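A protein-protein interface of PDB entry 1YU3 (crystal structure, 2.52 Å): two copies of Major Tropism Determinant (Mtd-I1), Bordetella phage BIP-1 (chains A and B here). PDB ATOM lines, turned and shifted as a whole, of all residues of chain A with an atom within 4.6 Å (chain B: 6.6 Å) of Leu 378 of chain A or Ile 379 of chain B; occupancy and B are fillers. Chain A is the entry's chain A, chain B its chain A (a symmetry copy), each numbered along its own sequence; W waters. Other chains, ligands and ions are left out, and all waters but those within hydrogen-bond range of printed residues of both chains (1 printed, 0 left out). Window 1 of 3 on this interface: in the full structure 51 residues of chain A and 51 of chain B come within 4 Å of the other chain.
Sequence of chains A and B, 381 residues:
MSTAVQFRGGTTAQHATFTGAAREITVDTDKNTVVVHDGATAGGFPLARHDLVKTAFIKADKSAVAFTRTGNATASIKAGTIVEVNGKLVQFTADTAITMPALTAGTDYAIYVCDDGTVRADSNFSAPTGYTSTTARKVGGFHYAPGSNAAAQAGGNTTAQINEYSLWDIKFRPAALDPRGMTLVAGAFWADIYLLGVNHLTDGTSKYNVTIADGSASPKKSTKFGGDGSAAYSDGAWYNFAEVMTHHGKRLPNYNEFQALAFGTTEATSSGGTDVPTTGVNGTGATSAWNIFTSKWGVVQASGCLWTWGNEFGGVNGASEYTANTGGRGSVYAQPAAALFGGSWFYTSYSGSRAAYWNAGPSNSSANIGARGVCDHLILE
The backbone carbonyl oxygen (O) of Lys 171 of chain A sits at hydrogen-bond distance from the backbone NH (N) of Leu 380 of chain A, at 2.9 Å. O of Lys 171 of chain B lies within hydrogen-bond range of N of Leu 380 of chain B, at 2.9 Å. The backbone NH (N) of Leu 378 of chain A sits at hydrogen-bond distance from the backbone carbonyl oxygen (O) of Arg 173 of chain A (2.9 Å).
Among the printed residues, pairs that only touch across the chains: Leu 378 of chain A with Ile 379 of chain B (3.8 Å) and Leu 380 of chain A with Leu 380 of chain B (3.8 Å).
Of the 10 printed residues of chain A, 2 touch a printed residue of chain B. Hydrophobic or aromatic side chains of chain A within 4 Å of the printed part of chain B: Leu 378 and Leu 380. Along chain A the printed residues that touch a printed residue of chain B span positions 378 to 380. Of the 11 printed residues of chain B, 2 touch a printed residue of chain A. Hydrophobic or aromatic side chains of chain B within 4 Å of the printed part of chain A: Leu 380.
Asp 376 of chain A touches none of the printed residues of chain B. Leu 378 of chain A touches one residue of chain B. Of the printed residues of chain B, Leu 380 of chain A touches Leu 380 (3.8 Å). Gly 187 of chain B touches none of the printed residues of chain A. Printed residues of chain A within 4 Å of Ile 379 of chain B: Leu 378. Of the printed residues of chain A, Leu 380 of chain B touches Leu 380. The nearest residue of chain B that does not touch Leu 378 of chain A is Leu 378 of chain B (5.7 Å).
Water W1 lies within hydrogen-bond range of NE of Arg 173 of chain A (3.4 Å) and O of Ile 379 of chain B (3.5 Å).
Leu 378 of chain A touches Ile 379 of chain B, but with the chains exchanged Ile 379 of chain A does not touch Leu 378 of chain B (9.1 Å). Leu 380 of chain B touches its own counterpart, Leu 380 of chain A. 7 positions are printed for both chains. Of the 2 pairs that touch across the chains among the printed residues, 1 has its exchanged pair printed and touching as well.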
ATOM      1  N   LYS A 171      14.502  10.423  20.741  1.00  0.00           N
ATOM      2  CA  LYS A 171      14.353  11.414  21.816  1.00  0.00           C
ATOM      3  C   LYS A 171      14.756  10.879  23.209  1.00  0.00           C
ATOM      4  O   LYS A 171      14.457  11.498  24.234  1.00  0.00           O
ATOM      5  CB  LYS A 171      12.924  11.967  21.825  1.00  0.00           C
ATOM      6  CG  LYS A 171      12.499  12.519  20.477  1.00  0.00           C
ATOM      7  CD  LYS A 171      11.455  13.597  20.601  1.00  0.00           C
ATOM      8  CE  LYS A 171      11.142  14.190  19.241  1.00  0.00           C
ATOM      9  NZ  LYS A 171       9.956  15.070  19.334  1.00  0.00           N
ATOM     10  N   PHE A 172      15.453   9.740  23.224  1.00  0.00           N
ATOM     11  CA  PHE A 172      15.811   9.019  24.442  1.00  0.00           C
ATOM     12  C   PHE A 172      16.999   8.135  24.060  1.00  0.00           C
ATOM     13  O   PHE A 172      16.825   6.970  23.680  1.00  0.00           O
ATOM     14  CB  PHE A 172      14.627   8.164  24.901  1.00  0.00           C
ATOM     15  CG  PHE A 172      14.753   7.631  26.309  1.00  0.00           C
ATOM     16  CD1 PHE A 172      14.214   8.333  27.383  1.00  0.00           C
ATOM     17  CD2 PHE A 172      15.389   6.418  26.555  1.00  0.00           C
ATOM     18  CE1 PHE A 172      14.317   7.836  28.680  1.00  0.00           C
ATOM     19  CE2 PHE A 172      15.489   5.913  27.847  1.00  0.00           C
ATOM     20  CZ  PHE A 172      14.954   6.623  28.909  1.00  0.00           C
ATOM     21  N   ARG A 173      18.203   8.700  24.156  1.00  0.00           N
ATOM     22  CA  ARG A 173      19.369   8.162  23.462  1.00  0.00           C
ATOM     23  C   ARG A 173      20.679   8.649  24.088  1.00  0.00           C
ATOM     24  O   ARG A 173      20.675   9.629  24.835  1.00  0.00           O
ATOM     25  CB  ARG A 173      19.320   8.590  21.990  1.00  0.00           C
ATOM     26  CG  ARG A 173      19.271  10.113  21.803  1.00  0.00           C
ATOM     27  CD  ARG A 173      19.256  10.523  20.347  1.00  0.00           C
ATOM     28  NE  ARG A 173      20.486  10.118  19.681  1.00  0.00           N
ATOM     29  CZ  ARG A 173      20.598   9.866  18.374  1.00  0.00           C
ATOM     30  NH1 ARG A 173      19.539   9.981  17.562  1.00  0.00           N
ATOM     31  NH2 ARG A 173      21.780   9.495  17.874  1.00  0.00           N
ATOM     32  N   ALA A 175      24.115  10.720  24.081  1.00  0.00           N
ATOM     33  CA  ALA A 175      24.604  11.946  23.454  1.00  0.00           C
ATOM     34  C   ALA A 175      25.788  11.658  22.524  1.00  0.00           C
ATOM     35  O   ALA A 175      26.190  12.518  21.747  1.00  0.00           O
ATOM     36  CB  ALA A 175      24.982  12.987  24.510  1.00  0.00           C
ATOM     37  N   TRP A 190      24.819   6.691  29.543  1.00  0.00           N
ATOM     38  CA  TRP A 190      25.029   5.506  28.709  1.00  0.00           C
ATOM     39  C   TRP A 190      26.457   4.980  28.812  1.00  0.00           C
ATOM     40  O   TRP A 190      27.417   5.762  28.887  1.00  0.00           O
ATOM     41  CB  TRP A 190      24.668   5.784  27.249  1.00  0.00           C
ATOM     42  CG  TRP A 190      23.234   6.106  27.053  1.00  0.00           C
ATOM     43  CD1 TRP A 190      22.624   7.289  27.319  1.00  0.00           C
ATOM     44  CD2 TRP A 190      22.214   5.229  26.550  1.00  0.00           C
ATOM     45  NE1 TRP A 190      21.290   7.214  27.017  1.00  0.00           N
ATOM     46  CE2 TRP A 190      21.007   5.961  26.542  1.00  0.00           C
ATOM     47  CE3 TRP A 190      22.205   3.897  26.097  1.00  0.00           C
ATOM     48  CZ2 TRP A 190      19.799   5.411  26.098  1.00  0.00           C
ATOM     49  CZ3 TRP A 190      21.011   3.348  25.664  1.00  0.00           C
ATOM     50  CH2 TRP A 190      19.818   4.108  25.666  1.00  0.00           C
ATOM     51  N   ASP A 376      26.519  11.139  28.100  1.00  0.00           N
ATOM     52  CA  ASP A 376      25.340  11.643  28.773  1.00  0.00           C
ATOM     53  C   ASP A 376      24.074  11.020  28.207  1.00  0.00           C
ATOM     54  O   ASP A 376      24.031  10.599  27.048  1.00  0.00           O
ATOM     55  CB  ASP A 376      25.286  13.174  28.660  1.00  0.00           C
ATOM     56  CG  ASP A 376      26.311  13.865  29.546  1.00  0.00           C
ATOM     57  OD1 ASP A 376      27.178  13.183  30.136  1.00  0.00           O
ATOM     58  OD2 ASP A 376      26.249  15.105  29.667  1.00  0.00           O
ATOM     59  N   HIS A 377      23.048  10.956  29.044  1.00  0.00           N
ATOM     60  CA  HIS A 377      21.735  10.541  28.599  1.00  0.00           C
ATOM     61  C   HIS A 377      20.944  11.745  28.067  1.00  0.00           C
ATOM     62  O   HIS A 377      20.855  12.776  28.728  1.00  0.00           O
ATOM     63  CB  HIS A 377      20.978   9.842  29.733  1.00  0.00           C
ATOM     64  CG  HIS A 377      19.641   9.308  29.321  1.00  0.00           C
ATOM     65  ND1 HIS A 377      18.560   9.268  30.174  1.00  0.00           N
ATOM     66  CD2 HIS A 377      19.203   8.816  28.136  1.00  0.00           C
ATOM     67  CE1 HIS A 377      17.519   8.761  29.538  1.00  0.00           C
ATOM     68  NE2 HIS A 377      17.882   8.481  28.299  1.00  0.00           N
ATOM     69  N   LEU A 378      20.369  11.602  26.874  1.00  0.00           N
ATOM     70  CA  LEU A 378      19.612  12.680  26.244  1.00  0.00           C
ATOM     71  C   LEU A 378      18.109  12.385  26.185  1.00  0.00           C
ATOM     72  O   LEU A 378      17.689  11.410  25.561  1.00  0.00           O
ATOM     73  CB  LEU A 378      20.148  12.918  24.836  1.00  0.00           C
ATOM     74  CG  LEU A 378      20.445  14.347  24.384  1.00  0.00           C
ATOM     75  CD1 LEU A 378      21.614  14.937  25.192  1.00  0.00           C
ATOM     76  CD2 LEU A 378      20.764  14.357  22.879  1.00  0.00           C
ATOM     77  N   ILE A 379      17.312  13.224  26.847  1.00  0.00           N
ATOM     78  CA  ILE A 379      15.847  13.135  26.822  1.00  0.00           C
ATOM     79  C   ILE A 379      15.281  14.395  26.160  1.00  0.00           C
ATOM     80  O   ILE A 379      15.406  15.490  26.720  1.00  0.00           O
ATOM     81  CB  ILE A 379      15.252  12.981  28.260  1.00  0.00           C
ATOM     82  CG1 ILE A 379      15.676  11.651  28.894  1.00  0.00           C
ATOM     83  CG2 ILE A 379      13.729  13.065  28.233  1.00  0.00           C
ATOM     84  CD1 ILE A 379      15.319  11.508  30.381  1.00  0.00           C
ATOM     85  N   LEU A 380      14.650  14.246  24.993  1.00  0.00           N
ATOM     86  CA  LEU A 380      14.235  15.393  24.168  1.00  0.00           C
ATOM     87  C   LEU A 380      12.743  15.446  23.897  1.00  0.00           C
ATOM     88  O   LEU A 380      11.947  15.638  24.803  1.00  0.00           O
ATOM     89  CB  LEU A 380      14.956  15.374  22.818  1.00  0.00           C
ATOM     90  CG  LEU A 380      16.474  15.232  22.768  1.00  0.00           C
ATOM     91  CD1 LEU A 380      16.947  15.037  21.329  1.00  0.00           C
ATOM     92  CD2 LEU A 380      17.125  16.441  23.384  1.00  0.00           C
ATOM     93  N   LYS B  62      20.103  15.478  10.999  1.00  0.00           N
ATOM     94  CA  LYS B  62      19.983  16.144  12.291  1.00  0.00           C
ATOM     95  C   LYS B  62      21.237  15.993  13.125  1.00  0.00           C
ATOM     96  O   LYS B  62      21.369  16.630  14.164  1.00  0.00           O
ATOM     97  CB  LYS B  62      18.772  15.630  13.054  1.00  0.00           C
ATOM     98  CG  LYS B  62      17.474  15.882  12.322  1.00  0.00           C
ATOM     99  CD  LYS B  62      16.302  15.780  13.263  1.00  0.00           C
ATOM    100  CE  LYS B  62      14.996  16.094  12.558  1.00  0.00           C
ATOM    101  NZ  LYS B  62      13.960  16.449  13.568  1.00  0.00           N
ATOM    102  N   SER B  63      22.160  15.162  12.649  1.00  0.00           N
ATOM    103  CA  SER B  63      23.408  14.918  13.344  1.00  0.00           C
ATOM    104  C   SER B  63      24.560  15.800  12.831  1.00  0.00           C
ATOM    105  O   SER B  63      25.691  15.654  13.283  1.00  0.00           O
ATOM    106  CB  SER B  63      23.778  13.442  13.226  1.00  0.00           C
ATOM    107  OG  SER B  63      24.402  13.198  11.979  1.00  0.00           O
ATOM    108  N   ALA B  64      24.274  16.696  11.886  1.00  0.00           N
ATOM    109  CA  ALA B  64      25.264  17.668  11.415  1.00  0.00           C
ATOM    110  C   ALA B  64      24.688  19.084  11.406  1.00  0.00           C
ATOM    111  O   ALA B  64      23.465  19.261  11.413  1.00  0.00           O
ATOM    112  CB  ALA B  64      25.789  17.284  10.028  1.00  0.00           C
ATOM    113  N   LYS B 171      19.691  23.870  16.489  1.00  0.00           N
ATOM    114  CA  LYS B 171      19.597  22.477  16.946  1.00  0.00           C
ATOM    115  C   LYS B 171      20.954  21.736  16.950  1.00  0.00           C
ATOM    116  O   LYS B 171      21.002  20.509  17.066  1.00  0.00           O
ATOM    117  CB  LYS B 171      18.554  21.722  16.115  1.00  0.00           C
ATOM    118  CG  LYS B 171      17.202  22.410  16.102  1.00  0.00           C
ATOM    119  CD  LYS B 171      16.067  21.443  15.890  1.00  0.00           C
ATOM    120  CE  LYS B 171      14.735  22.160  15.992  1.00  0.00           C
ATOM    121  NZ  LYS B 171      13.643  21.264  15.549  1.00  0.00           N
ATOM    122  N   PHE B 172      22.043  22.501  16.843  1.00  0.00           N
ATOM    123  CA  PHE B 172      23.398  21.975  16.703  1.00  0.00           C
ATOM    124  C   PHE B 172      24.324  23.109  17.148  1.00  0.00           C
ATOM    125  O   PHE B 172      24.783  23.911  16.324  1.00  0.00           O
ATOM    126  CB  PHE B 172      23.658  21.606  15.240  1.00  0.00           C
ATOM    127  CG  PHE B 172      24.889  20.759  15.023  1.00  0.00           C
ATOM    128  CD1 PHE B 172      24.798  19.371  14.993  1.00  0.00           C
ATOM    129  CD2 PHE B 172      26.133  21.351  14.823  1.00  0.00           C
ATOM    130  CE1 PHE B 172      25.930  18.588  14.778  1.00  0.00           C
ATOM    131  CE2 PHE B 172      27.266  20.575  14.600  1.00  0.00           C
ATOM    132  CZ  PHE B 172      27.163  19.194  14.580  1.00  0.00           C
ATOM    133  N   ARG B 173      24.587  23.172  18.453  1.00  0.00           N
ATOM    134  CA  ARG B 173      25.094  24.387  19.084  1.00  0.00           C
ATOM    135  C   ARG B 173      25.769  24.092  20.427  1.00  0.00           C
ATOM    136  O   ARG B 173      25.561  23.020  20.995  1.00  0.00           O
ATOM    137  CB  ARG B 173      23.932  25.362  19.304  1.00  0.00           C
ATOM    138  CG  ARG B 173      22.801  24.774  20.160  1.00  0.00           C
ATOM    139  CD  ARG B 173      21.675  25.757  20.396  1.00  0.00           C
ATOM    140  NE  ARG B 173      22.143  26.908  21.157  1.00  0.00           N
ATOM    141  CZ  ARG B 173      21.599  28.128  21.106  1.00  0.00           C
ATOM    142  NH1 ARG B 173      20.541  28.373  20.321  1.00  0.00           N
ATOM    143  NH2 ARG B 173      22.117  29.110  21.847  1.00  0.00           N
ATOM    144  N   GLY B 187      33.536  17.094  16.826  1.00  0.00           N
ATOM    145  CA  GLY B 187      32.103  16.864  16.971  1.00  0.00           C
ATOM    146  C   GLY B 187      31.652  16.528  18.390  1.00  0.00           C
ATOM    147  O   GLY B 187      30.514  16.122  18.584  1.00  0.00           O
ATOM    148  N   HIS B 377      28.286  19.776  23.674  1.00  0.00           N
ATOM    149  CA  HIS B 377      27.668  19.888  22.370  1.00  0.00           C
ATOM    150  C   HIS B 377      26.189  19.481  22.440  1.00  0.00           C
ATOM    151  O   HIS B 377      25.857  18.425  22.970  1.00  0.00           O
ATOM    152  CB  HIS B 377      28.425  19.044  21.340  1.00  0.00           C
ATOM    153  CG  HIS B 377      27.893  19.177  19.947  1.00  0.00           C
ATOM    154  ND1 HIS B 377      27.898  18.136  19.045  1.00  0.00           N
ATOM    155  CD2 HIS B 377      27.314  20.224  19.310  1.00  0.00           C
ATOM    156  CE1 HIS B 377      27.360  18.540  17.908  1.00  0.00           C
ATOM    157  NE2 HIS B 377      26.995  19.803  18.043  1.00  0.00           N
ATOM    158  N   LEU B 378      25.311  20.323  21.897  1.00  0.00           N
ATOM    159  CA  LEU B 378      23.873  20.065  21.922  1.00  0.00           C
ATOM    160  C   LEU B 378      23.312  19.743  20.531  1.00  0.00           C
ATOM    161  O   LEU B 378      23.385  20.571  19.623  1.00  0.00           O
ATOM    162  CB  LEU B 378      23.154  21.278  22.502  1.00  0.00           C
ATOM    163  CG  LEU B 378      22.095  21.068  23.585  1.00  0.00           C
ATOM    164  CD1 LEU B 378      22.742  20.529  24.873  1.00  0.00           C
ATOM    165  CD2 LEU B 378      21.364  22.393  23.856  1.00  0.00           C
ATOM    166  N   ILE B 379      22.766  18.537  20.377  1.00  0.00           N
ATOM    167  CA  ILE B 379      22.107  18.102  19.139  1.00  0.00           C
ATOM    168  C   ILE B 379      20.624  17.849  19.426  1.00  0.00           C
ATOM    169  O   ILE B 379      20.293  16.917  20.167  1.00  0.00           O
ATOM    170  CB  ILE B 379      22.761  16.806  18.560  1.00  0.00           C
ATOM    171  CG1 ILE B 379      24.206  17.065  18.118  1.00  0.00           C
ATOM    172  CG2 ILE B 379      21.960  16.270  17.378  1.00  0.00           C
ATOM    173  CD1 ILE B 379      24.997  15.804  17.738  1.00  0.00           C
ATOM    174  N   LEU B 380      19.738  18.654  18.834  1.00  0.00           N
ATOM    175  CA  LEU B 380      18.305  18.638  19.176  1.00  0.00           C
ATOM    176  C   LEU B 380      17.397  18.327  18.002  1.00  0.00           C
ATOM    177  O   LEU B 380      17.418  17.229  17.466  1.00  0.00           O
ATOM    178  CB  LEU B 380      17.876  19.988  19.756  1.00  0.00           C
ATOM    179  CG  LEU B 380      18.668  20.611  20.900  1.00  0.00           C
ATOM    180  CD1 LEU B 380      18.183  22.034  21.176  1.00  0.00           C
ATOM    181  CD2 LEU B 380      18.548  19.759  22.134  1.00  0.00           C
HETATM  182  O   HOH W   1      20.254  13.529  19.474  1.00  0.00           O
